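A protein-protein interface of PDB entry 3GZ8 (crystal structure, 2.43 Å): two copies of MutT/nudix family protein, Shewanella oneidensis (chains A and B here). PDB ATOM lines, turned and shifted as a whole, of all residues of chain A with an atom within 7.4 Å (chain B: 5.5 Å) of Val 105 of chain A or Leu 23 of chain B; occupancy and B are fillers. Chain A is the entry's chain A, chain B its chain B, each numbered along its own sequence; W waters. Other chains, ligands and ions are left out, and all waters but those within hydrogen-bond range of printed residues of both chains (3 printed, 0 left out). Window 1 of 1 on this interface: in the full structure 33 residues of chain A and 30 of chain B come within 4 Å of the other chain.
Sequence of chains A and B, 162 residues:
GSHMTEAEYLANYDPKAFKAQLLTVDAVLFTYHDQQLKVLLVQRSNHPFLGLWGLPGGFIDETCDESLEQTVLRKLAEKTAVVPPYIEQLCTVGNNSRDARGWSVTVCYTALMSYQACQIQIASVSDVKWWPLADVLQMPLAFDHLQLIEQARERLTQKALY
The backbone NH (N) of Leu 68 of chain B sits at hydrogen-bond distance from the backbone carbonyl oxygen (O) of Gly 94 of chain A, 3.0 Å away.
O of Trp 103 of chain A lies within hydrogen-bond range of N of Leu 22 of chain A (2.9 Å).
The backbone carbonyl oxygen (O) of Leu 22 of chain A sits at hydrogen-bond distance from the backbone NH (N) of Val 105 of chain A (2.8 Å).
N of Thr 24 of chain A sits at hydrogen-bond distance from O of Val 105 of chain A (2.9 Å).
The backbone carbonyl oxygen (O) of Leu 22 of chain B is in hydrogen-bond range of the backbone NH (N) of Val 105 of chain B, at 2.9 Å.
The backbone NH (N) of Thr 24 of chain B sits at hydrogen-bond distance from the backbone carbonyl oxygen (O) of Val 105 of chain B (3.0 Å).
The backbone carbonyl oxygen of Thr 24 of chain B lies within hydrogen-bond range of the backbone NH of Val 107 of chain B (3.0 Å).
Gln 21 of chain A touches Leu 23 of chain B (OE1 to CD2, 3.5 Å).
Ile 60 of chain B touches Gln 21 of chain A.
Leu 23 of chain A touches Gln 21 of chain B (CD2 to CB, 3.8 Å).
Val 105 of chain B touches Leu 23 of chain A.
Leu 68 of chain B touches Thr 92 of chain A (CD1 to CG2, 3.8 Å).
Val 107 of chain B touches Thr 92 of chain A.
Trp 103 of chain A touches Ile 60 of chain B.
N of Leu 68 of chain B touches CH2 of Trp 103 of chain A, 3.7 Å away.
Leu 23 of chain B touches Val 105 of chain A (CD2 to CG2, 3.5 Å).
Leu 68 of chain B touches Val 105 of chain A (CD2 to CG2, 3.96 Å).
Val 105 of chain A touches just these residues of chain B: Leu 23 and Leu 68.
Leu 23 of chain B touches just these residues of chain A: Gln 21 (3.5 Å) and Val 105 (3.5 Å).
Of the printed residues of chain B, Trp 103 of chain A touches Ile 60 (3.6 Å) and Leu 68 (3.7 Å).
Of the printed residues of chain B, Gln 21 of chain A touches Leu 23 (3.5 Å) and Ile 60 (3.8 Å).
Of the printed residues of chain A, Gln 21 of chain B touches Leu 23.
Cys 108 of chain A touches none of the printed residues of chain B.
Thr 24 of chain B touches none of the printed residues of chain A.
The nearest residue of chain B that does not touch Val 105 of chain A is Ile 60 of chain B (4.5 Å).
The nearest residue of chain A that does not touch Leu 23 of chain B is Leu 23 of chain A (4.4 Å).
The nearest printed residue of chain A that does not touch Val 107 of chain B is Val 105 of chain A (4.8 Å).
Of the 22 printed residues of chain A, 6 touch a printed residue of chain B.
Hydrophobic or aromatic side chains of chain A that line the printed part of chain B: Leu 23, Trp 103 and Val 105.
Gln 21 of chain A touches Leu 23 of chain B, and with the chains exchanged Leu 23 of chain A touches Gln 21 of chain B.
Leu 23 of chain A touches Val 105 of chain B, and with the chains exchanged Val 105 of chain A touches Leu 23 of chain B.
Positions printed for both chains: 21, 22, 23, 24, 25, 58, 59, 105 and 107.
Water W3 bridges the side-chain amide oxygen of Gln 21 of chain B (2.5 Å) and the backbone carbonyl oxygen of Leu 23 of chain A (2.7 Å).
Water W1 lies within hydrogen-bond range of the backbone carbonyl oxygen of Leu 23 of chain B (2.7 Å), the side-chain amide oxygen of Gln 21 of chain A (2.7 Å) and the backbone NH of Ile 60 of chain B (3.2 Å).
Water W2 bridges N of Gln 21 of chain A (2.9 Å) and O of Gln 21 of chain B (3.0 Å).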
ATOM      1  N   ALA A  20     -14.528  20.032 -24.570  1.00  0.00           N
ATOM      2  CA  ALA A  20     -15.306  21.222 -24.285  1.00  0.00           C
ATOM      3  C   ALA A  20     -15.416  22.076 -25.540  1.00  0.00           C
ATOM      4  O   ALA A  20     -14.670  21.893 -26.497  1.00  0.00           O
ATOM      5  CB  ALA A  20     -14.684  22.010 -23.160  1.00  0.00           C
ATOM      6  N   GLN A  21     -16.364  23.001 -25.519  1.00  0.00           N
ATOM      7  CA  GLN A  21     -16.626  23.884 -26.641  1.00  0.00           C
ATOM      8  C   GLN A  21     -16.120  25.275 -26.270  1.00  0.00           C
ATOM      9  O   GLN A  21     -15.784  25.508 -25.103  1.00  0.00           O
ATOM     10  CB  GLN A  21     -18.132  23.897 -26.912  1.00  0.00           C
ATOM     11  CG  GLN A  21     -18.665  22.564 -27.434  1.00  0.00           C
ATOM     12  CD  GLN A  21     -18.934  21.535 -26.352  1.00  0.00           C
ATOM     13  OE1 GLN A  21     -19.363  21.864 -25.246  1.00  0.00           O
ATOM     14  NE2 GLN A  21     -18.689  20.275 -26.671  1.00  0.00           N
ATOM     15  N   LEU A  22     -16.041  26.189 -27.236  1.00  0.00           N
ATOM     16  CA  LEU A  22     -15.715  27.588 -26.915  1.00  0.00           C
ATOM     17  C   LEU A  22     -16.934  28.275 -26.376  1.00  0.00           C
ATOM     18  O   LEU A  22     -18.036  28.089 -26.887  1.00  0.00           O
ATOM     19  CB  LEU A  22     -15.240  28.376 -28.133  1.00  0.00           C
ATOM     20  CG  LEU A  22     -13.973  27.991 -28.910  1.00  0.00           C
ATOM     21  CD1 LEU A  22     -13.475  29.269 -29.575  1.00  0.00           C
ATOM     22  CD2 LEU A  22     -12.858  27.384 -28.055  1.00  0.00           C
ATOM     23  N   LEU A  23     -16.730  29.091 -25.352  1.00  0.00           N
ATOM     24  CA  LEU A  23     -17.817  29.768 -24.677  1.00  0.00           C
ATOM     25  C   LEU A  23     -17.483  31.229 -24.594  1.00  0.00           C
ATOM     26  O   LEU A  23     -16.443  31.605 -24.043  1.00  0.00           O
ATOM     27  CB  LEU A  23     -17.942  29.185 -23.290  1.00  0.00           C
ATOM     28  CG  LEU A  23     -19.150  29.382 -22.380  1.00  0.00           C
ATOM     29  CD1 LEU A  23     -20.451  29.749 -23.129  1.00  0.00           C
ATOM     30  CD2 LEU A  23     -19.313  28.061 -21.605  1.00  0.00           C
ATOM     31  N   THR A  24     -18.344  32.064 -25.169  1.00  0.00           N
ATOM     32  CA  THR A  24     -18.066  33.489 -25.242  1.00  0.00           C
ATOM     33  C   THR A  24     -19.307  34.305 -24.950  1.00  0.00           C
ATOM     34  O   THR A  24     -20.417  33.758 -24.846  1.00  0.00           O
ATOM     35  CB  THR A  24     -17.507  33.890 -26.629  1.00  0.00           C
ATOM     36  OG1 THR A  24     -18.399  33.467 -27.662  1.00  0.00           O
ATOM     37  CG2 THR A  24     -16.120  33.255 -26.887  1.00  0.00           C
ATOM     38  N   VAL A  25     -19.104  35.613 -24.788  1.00  0.00           N
ATOM     39  CA  VAL A  25     -20.199  36.574 -24.735  1.00  0.00           C
ATOM     40  C   VAL A  25     -19.959  37.627 -25.797  1.00  0.00           C
ATOM     41  O   VAL A  25     -18.814  37.817 -26.223  1.00  0.00           O
ATOM     42  CB  VAL A  25     -20.360  37.243 -23.345  1.00  0.00           C
ATOM     43  CG1 VAL A  25     -20.551  36.204 -22.261  1.00  0.00           C
ATOM     44  CG2 VAL A  25     -19.185  38.146 -23.027  1.00  0.00           C
ATOM     45  N   ASP A  26     -21.016  38.306 -26.230  1.00  0.00           N
ATOM     46  CA  ASP A  26     -20.891  39.417 -27.177  1.00  0.00           C
ATOM     47  C   ASP A  26     -21.895  40.470 -26.763  1.00  0.00           C
ATOM     48  O   ASP A  26     -22.889  40.140 -26.111  1.00  0.00           O
ATOM     49  CB  ASP A  26     -21.202  38.960 -28.600  1.00  0.00           C
ATOM     50  CG  ASP A  26     -20.029  38.273 -29.270  1.00  0.00           C
ATOM     51  OD1 ASP A  26     -18.980  38.919 -29.462  1.00  0.00           O
ATOM     52  OD2 ASP A  26     -20.165  37.096 -29.631  1.00  0.00           O
ATOM     53  N   GLY A  58     -15.880  38.256 -25.812  1.00  0.00           N
ATOM     54  CA  GLY A  58     -14.773  37.587 -25.169  1.00  0.00           C
ATOM     55  C   GLY A  58     -15.075  36.363 -24.340  1.00  0.00           C
ATOM     56  O   GLY A  58     -16.227  35.898 -24.258  1.00  0.00           O
ATOM     57  N   PHE A  59     -14.018  35.853 -23.713  1.00  0.00           N
ATOM     58  CA  PHE A  59     -14.075  34.634 -22.928  1.00  0.00           C
ATOM     59  C   PHE A  59     -14.271  34.897 -21.449  1.00  0.00           C
ATOM     60  O   PHE A  59     -13.837  35.930 -20.902  1.00  0.00           O
ATOM     61  CB  PHE A  59     -12.787  33.845 -23.118  1.00  0.00           C
ATOM     62  CG  PHE A  59     -12.597  33.336 -24.512  1.00  0.00           C
ATOM     63  CD1 PHE A  59     -13.146  32.115 -24.888  1.00  0.00           C
ATOM     64  CD2 PHE A  59     -11.872  34.083 -25.450  1.00  0.00           C
ATOM     65  CE1 PHE A  59     -12.973  31.626 -26.173  1.00  0.00           C
ATOM     66  CE2 PHE A  59     -11.704  33.624 -26.741  1.00  0.00           C
ATOM     67  CZ  PHE A  59     -12.242  32.376 -27.112  1.00  0.00           C
ATOM     68  N   THR A  92     -28.607  33.369 -27.714  1.00  0.00           N
ATOM     69  CA  THR A  92     -27.449  32.522 -27.638  1.00  0.00           C
ATOM     70  C   THR A  92     -27.331  31.761 -28.963  1.00  0.00           C
ATOM     71  O   THR A  92     -28.256  31.075 -29.385  1.00  0.00           O
ATOM     72  CB  THR A  92     -27.572  31.583 -26.437  1.00  0.00           C
ATOM     73  OG1 THR A  92     -27.584  32.374 -25.235  1.00  0.00           O
ATOM     74  CG2 THR A  92     -26.415  30.571 -26.376  1.00  0.00           C
ATOM     75  N   VAL A  93     -26.211  31.941 -29.645  1.00  0.00           N
ATOM     76  CA  VAL A  93     -25.960  31.231 -30.887  1.00  0.00           C
ATOM     77  C   VAL A  93     -24.868  30.179 -30.646  1.00  0.00           C
ATOM     78  O   VAL A  93     -23.802  30.490 -30.118  1.00  0.00           O
ATOM     79  CB  VAL A  93     -25.574  32.181 -32.054  1.00  0.00           C
ATOM     80  CG1 VAL A  93     -25.362  31.373 -33.364  1.00  0.00           C
ATOM     81  CG2 VAL A  93     -26.670  33.278 -32.269  1.00  0.00           C
ATOM     82  N   GLY A  94     -25.160  28.930 -31.001  1.00  0.00           N
ATOM     83  CA  GLY A  94     -24.250  27.831 -30.757  1.00  0.00           C
ATOM     84  C   GLY A  94     -24.256  26.816 -31.863  1.00  0.00           C
ATOM     85  O   GLY A  94     -25.245  26.117 -32.062  1.00  0.00           O
ATOM     86  N   ASN A  95     -23.146  26.715 -32.577  1.00  0.00           N
ATOM     87  CA  ASN A  95     -23.030  25.722 -33.648  1.00  0.00           C
ATOM     88  C   ASN A  95     -21.568  25.436 -34.009  1.00  0.00           C
ATOM     89  O   ASN A  95     -20.636  25.986 -33.390  1.00  0.00           O
ATOM     90  CB  ASN A  95     -23.814  26.178 -34.885  1.00  0.00           C
ATOM     91  CG  ASN A  95     -23.289  27.468 -35.445  1.00  0.00           C
ATOM     92  OD1 ASN A  95     -22.058  27.656 -35.573  1.00  0.00           O
ATOM     93  ND2 ASN A  95     -24.200  28.386 -35.776  1.00  0.00           N
ATOM     94  N   ARG A  98     -19.784  28.850 -36.857  1.00  0.00           N
ATOM     95  CA  ARG A  98     -19.656  30.305 -36.680  1.00  0.00           C
ATOM     96  C   ARG A  98     -18.207  30.743 -36.318  1.00  0.00           C
ATOM     97  O   ARG A  98     -17.806  31.897 -36.567  1.00  0.00           O
ATOM     98  CB  ARG A  98     -20.687  30.825 -35.656  1.00  0.00           C
ATOM     99  CG  ARG A  98     -20.551  30.225 -34.242  1.00  0.00           C
ATOM    100  CD  ARG A  98     -21.444  30.911 -33.167  1.00  0.00           C
ATOM    101  NE  ARG A  98     -21.233  32.352 -33.185  1.00  0.00           N
ATOM    102  CZ  ARG A  98     -20.266  32.999 -32.530  1.00  0.00           C
ATOM    103  NH1 ARG A  98     -19.413  32.341 -31.736  1.00  0.00           N
ATOM    104  NH2 ARG A  98     -20.174  34.324 -32.648  1.00  0.00           N
ATOM    105  N   ASP A  99     -17.442  29.821 -35.724  1.00  0.00           N
ATOM    106  CA  ASP A  99     -16.086  30.096 -35.249  1.00  0.00           C
ATOM    107  C   ASP A  99     -15.150  28.978 -35.704  1.00  0.00           C
ATOM    108  O   ASP A  99     -15.235  27.837 -35.221  1.00  0.00           O
ATOM    109  CB  ASP A  99     -16.067  30.215 -33.715  1.00  0.00           C
ATOM    110  CG  ASP A  99     -14.840  30.965 -33.184  1.00  0.00           C
ATOM    111  OD1 ASP A  99     -13.693  30.683 -33.601  1.00  0.00           O
ATOM    112  OD2 ASP A  99     -15.016  31.858 -32.331  1.00  0.00           O
ATOM    113  N   GLY A 102     -13.449  26.141 -33.568  1.00  0.00           N
ATOM    114  CA  GLY A 102     -14.138  24.919 -33.089  1.00  0.00           C
ATOM    115  C   GLY A 102     -15.613  25.179 -32.781  1.00  0.00           C
ATOM    116  O   GLY A 102     -16.100  26.334 -32.907  1.00  0.00           O
ATOM    117  N   TRP A 103     -16.308  24.104 -32.396  1.00  0.00           N
ATOM    118  CA  TRP A 103     -17.668  24.168 -31.872  1.00  0.00           C
ATOM    119  C   TRP A 103     -17.785  25.328 -30.864  1.00  0.00           C
ATOM    120  O   TRP A 103     -16.980  25.454 -29.933  1.00  0.00           O
ATOM    121  CB  TRP A 103     -18.045  22.837 -31.222  1.00  0.00           C
ATOM    122  CG  TRP A 103     -19.456  22.339 -31.559  1.00  0.00           C
ATOM    123  CD1 TRP A 103     -19.778  21.321 -32.400  1.00  0.00           C
ATOM    124  CD2 TRP A 103     -20.704  22.832 -31.039  1.00  0.00           C
ATOM    125  NE1 TRP A 103     -21.140  21.140 -32.434  1.00  0.00           N
ATOM    126  CE2 TRP A 103     -21.731  22.048 -31.604  1.00  0.00           C
ATOM    127  CE3 TRP A 103     -21.052  23.851 -30.141  1.00  0.00           C
ATOM    128  CZ2 TRP A 103     -23.095  22.266 -31.319  1.00  0.00           C
ATOM    129  CZ3 TRP A 103     -22.406  24.069 -29.864  1.00  0.00           C
ATOM    130  CH2 TRP A 103     -23.406  23.286 -30.454  1.00  0.00           C
ATOM    131  N   SER A 104     -18.771  26.193 -31.063  1.00  0.00           N
ATOM    132  CA  SER A 104     -18.724  27.487 -30.403  1.00  0.00           C
ATOM    133  C   SER A 104     -20.076  27.946 -29.910  1.00  0.00           C
ATOM    134  O   SER A 104     -21.044  27.855 -30.649  1.00  0.00           O
ATOM    135  CB  SER A 104     -18.196  28.512 -31.392  1.00  0.00           C
ATOM    136  OG  SER A 104     -18.603  29.824 -31.042  1.00  0.00           O
ATOM    137  N   VAL A 105     -20.124  28.466 -28.684  1.00  0.00           N
ATOM    138  CA  VAL A 105     -21.331  29.066 -28.130  1.00  0.00           C
ATOM    139  C   VAL A 105     -21.082  30.521 -27.737  1.00  0.00           C
ATOM    140  O   VAL A 105     -20.163  30.820 -26.980  1.00  0.00           O
ATOM    141  CB  VAL A 105     -21.852  28.305 -26.870  1.00  0.00           C
ATOM    142  CG1 VAL A 105     -23.037  29.049 -26.274  1.00  0.00           C
ATOM    143  CG2 VAL A 105     -22.265  26.866 -27.192  1.00  0.00           C
ATOM    144  N   THR A 106     -21.896  31.437 -28.234  1.00  0.00           N
ATOM    145  CA  THR A 106     -21.797  32.811 -27.742  1.00  0.00           C
ATOM    146  C   THR A 106     -23.142  33.280 -27.191  1.00  0.00           C
ATOM    147  O   THR A 106     -24.205  33.026 -27.768  1.00  0.00           O
ATOM    148  CB  THR A 106     -21.277  33.823 -28.818  1.00  0.00           C
ATOM    149  OG1 THR A 106     -20.779  35.006 -28.176  1.00  0.00           O
ATOM    150  CG2 THR A 106     -22.385  34.226 -29.795  1.00  0.00           C
ATOM    151  N   VAL A 107     -23.067  33.972 -26.067  1.00  0.00           N
ATOM    152  CA  VAL A 107     -24.249  34.527 -25.429  1.00  0.00           C
ATOM    153  C   VAL A 107     -24.264  36.015 -25.747  1.00  0.00           C
ATOM    154  O   VAL A 107     -23.444  36.754 -25.240  1.00  0.00           O
ATOM    155  CB  VAL A 107     -24.193  34.273 -23.901  1.00  0.00           C
ATOM    156  CG1 VAL A 107     -25.466  34.712 -23.228  1.00  0.00           C
ATOM    157  CG2 VAL A 107     -23.925  32.789 -23.625  1.00  0.00           C
ATOM    158  N   CYS A 108     -25.185  36.459 -26.594  1.00  0.00           N
ATOM    159  CA  CYS A 108     -25.192  37.861 -26.985  1.00  0.00           C
ATOM    160  C   CYS A 108     -26.103  38.704 -26.109  1.00  0.00           C
ATOM    161  O   CYS A 108     -27.204  38.291 -25.764  1.00  0.00           O
ATOM    162  CB  CYS A 108     -25.575  38.019 -28.473  1.00  0.00           C
ATOM    163  SG  CYS A 108     -25.135  39.662 -29.207  1.00  0.00           S
ATOM    164  N   GLN B  21     -15.335  25.911 -19.411  1.00  0.00           N
ATOM    165  CA  GLN B  21     -16.478  25.869 -18.532  1.00  0.00           C
ATOM    166  C   GLN B  21     -17.401  24.747 -18.972  1.00  0.00           C
ATOM    167  O   GLN B  21     -17.293  24.272 -20.104  1.00  0.00           O
ATOM    168  CB  GLN B  21     -17.228  27.220 -18.563  1.00  0.00           C
ATOM    169  CG  GLN B  21     -16.435  28.441 -18.021  1.00  0.00           C
ATOM    170  CD  GLN B  21     -15.304  28.885 -18.954  1.00  0.00           C
ATOM    171  OE1 GLN B  21     -15.511  29.085 -20.159  1.00  0.00           O
ATOM    172  NE2 GLN B  21     -14.102  29.025 -18.402  1.00  0.00           N
ATOM    173  N   LEU B  22     -18.296  24.324 -18.076  1.00  0.00           N
ATOM    174  CA  LEU B  22     -19.334  23.365 -18.406  1.00  0.00           C
ATOM    175  C   LEU B  22     -20.433  24.031 -19.201  1.00  0.00           C
ATOM    176  O   LEU B  22     -20.868  25.151 -18.887  1.00  0.00           O
ATOM    177  CB  LEU B  22     -19.958  22.741 -17.159  1.00  0.00           C
ATOM    178  CG  LEU B  22     -19.082  22.017 -16.116  1.00  0.00           C
ATOM    179  CD1 LEU B  22     -19.972  21.224 -15.172  1.00  0.00           C
ATOM    180  CD2 LEU B  22     -18.062  21.099 -16.768  1.00  0.00           C
ATOM    181  N   LEU B  23     -20.913  23.303 -20.208  1.00  0.00           N
ATOM    182  CA  LEU B  23     -21.878  23.815 -21.144  1.00  0.00           C
ATOM    183  C   LEU B  23     -22.944  22.780 -21.360  1.00  0.00           C
ATOM    184  O   LEU B  23     -22.633  21.640 -21.670  1.00  0.00           O
ATOM    185  CB  LEU B  23     -21.165  24.162 -22.439  1.00  0.00           C
ATOM    186  CG  LEU B  23     -21.860  24.543 -23.737  1.00  0.00           C
ATOM    187  CD1 LEU B  23     -22.961  25.590 -23.588  1.00  0.00           C
ATOM    188  CD2 LEU B  23     -20.761  25.059 -24.620  1.00  0.00           C
ATOM    189  N   THR B  24     -24.208  23.167 -21.189  1.00  0.00           N
ATOM    190  CA  THR B  24     -25.295  22.202 -21.254  1.00  0.00           C
ATOM    191  C   THR B  24     -26.503  22.854 -21.873  1.00  0.00           C
ATOM    192  O   THR B  24     -26.535  24.077 -22.016  1.00  0.00           O
ATOM    193  CB  THR B  24     -25.711  21.732 -19.850  1.00  0.00           C
ATOM    194  OG1 THR B  24     -26.061  22.875 -19.059  1.00  0.00           O
ATOM    195  CG2 THR B  24     -24.584  20.996 -19.159  1.00  0.00           C
ATOM    196  N   VAL B  25     -27.497  22.046 -22.222  1.00  0.00           N
ATOM    197  CA  VAL B  25     -28.799  22.546 -22.599  1.00  0.00           C
ATOM    198  C   VAL B  25     -29.840  22.019 -21.614  1.00  0.00           C
ATOM    199  O   VAL B  25     -29.551  21.138 -20.809  1.00  0.00           O
ATOM    200  CB  VAL B  25     -29.183  22.161 -24.061  1.00  0.00           C
ATOM    201  CG1 VAL B  25     -28.215  22.820 -25.088  1.00  0.00           C
ATOM    202  CG2 VAL B  25     -29.255  20.654 -24.234  1.00  0.00           C
ATOM    203  N   GLY B  58     -28.594  18.239 -20.951  1.00  0.00           N
ATOM    204  CA  GLY B  58     -27.362  17.510 -21.038  1.00  0.00           C
ATOM    205  C   GLY B  58     -26.318  18.202 -21.863  1.00  0.00           C
ATOM    206  O   GLY B  58     -26.464  19.393 -22.233  1.00  0.00           O
ATOM    207  N   PHE B  59     -25.266  17.444 -22.164  1.00  0.00           N
ATOM    208  CA  PHE B  59     -24.037  18.001 -22.725  1.00  0.00           C
ATOM    209  C   PHE B  59     -24.048  17.886 -24.233  1.00  0.00           C
ATOM    210  O   PHE B  59     -24.710  17.014 -24.794  1.00  0.00           O
ATOM    211  CB  PHE B  59     -22.821  17.275 -22.117  1.00  0.00           C
ATOM    212  CG  PHE B  59     -22.638  17.539 -20.643  1.00  0.00           C
ATOM    213  CD1 PHE B  59     -21.912  18.653 -20.202  1.00  0.00           C
ATOM    214  CD2 PHE B  59     -23.216  16.706 -19.703  1.00  0.00           C
ATOM    215  CE1 PHE B  59     -21.752  18.910 -18.840  1.00  0.00           C
ATOM    216  CE2 PHE B  59     -23.061  16.946 -18.351  1.00  0.00           C
ATOM    217  CZ  PHE B  59     -22.325  18.047 -17.908  1.00  0.00           C
ATOM    218  N   ILE B  60     -23.333  18.776 -24.900  1.00  0.00           N
ATOM    219  CA  ILE B  60     -23.228  18.695 -26.348  1.00  0.00           C
ATOM    220  C   ILE B  60     -22.424  17.456 -26.785  1.00  0.00           C
ATOM    221  O   ILE B  60     -21.426  17.090 -26.148  1.00  0.00           O
ATOM    222  CB  ILE B  60     -22.592  19.976 -26.905  1.00  0.00           C
ATOM    223  CG1 ILE B  60     -23.489  21.170 -26.570  1.00  0.00           C
ATOM    224  CG2 ILE B  60     -22.352  19.864 -28.410  1.00  0.00           C
ATOM    225  CD1 ILE B  60     -22.785  22.475 -26.668  1.00  0.00           C
ATOM    226  N   LEU B  68     -26.968  23.892 -31.069  1.00  0.00           N
ATOM    227  CA  LEU B  68     -27.615  23.771 -29.778  1.00  0.00           C
ATOM    228  C   LEU B  68     -29.026  23.191 -29.920  1.00  0.00           C
ATOM    229  O   LEU B  68     -29.429  22.326 -29.139  1.00  0.00           O
ATOM    230  CB  LEU B  68     -27.641  25.128 -29.069  1.00  0.00           C
ATOM    231  CG  LEU B  68     -26.310  25.728 -28.614  1.00  0.00           C
ATOM    232  CD1 LEU B  68     -26.507  27.164 -28.138  1.00  0.00           C
ATOM    233  CD2 LEU B  68     -25.676  24.884 -27.504  1.00  0.00           C
ATOM    234  N   VAL B 105     -22.675  27.050 -17.688  1.00  0.00           N
ATOM    235  CA  VAL B 105     -23.609  27.767 -18.519  1.00  0.00           C
ATOM    236  C   VAL B 105     -24.618  26.743 -19.027  1.00  0.00           C
ATOM    237  O   VAL B 105     -24.211  25.723 -19.595  1.00  0.00           O
ATOM    238  CB  VAL B 105     -22.913  28.405 -19.770  1.00  0.00           C
ATOM    239  CG1 VAL B 105     -23.942  29.003 -20.718  1.00  0.00           C
ATOM    240  CG2 VAL B 105     -21.862  29.432 -19.374  1.00  0.00           C
ATOM    241  N   VAL B 107     -28.190  26.494 -21.556  1.00  0.00           N
ATOM    242  CA  VAL B 107     -28.985  27.155 -22.566  1.00  0.00           C
ATOM    243  C   VAL B 107     -30.359  26.484 -22.540  1.00  0.00           C
ATOM    244  O   VAL B 107     -30.528  25.333 -22.948  1.00  0.00           O
ATOM    245  CB  VAL B 107     -28.344  27.067 -23.973  1.00  0.00           C
ATOM    246  CG1 VAL B 107     -29.114  27.893 -24.930  1.00  0.00           C
ATOM    247  CG2 VAL B 107     -26.907  27.568 -23.951  1.00  0.00           C
HETATM  248  O   HOH W   1     -21.046  20.577 -23.529  1.00  0.00           O
HETATM  249  O   HOH W   2     -17.753  23.619 -23.018  1.00  0.00           O
HETATM  250  O   HOH W   3     -15.035  30.912 -21.834  1.00  0.00           O
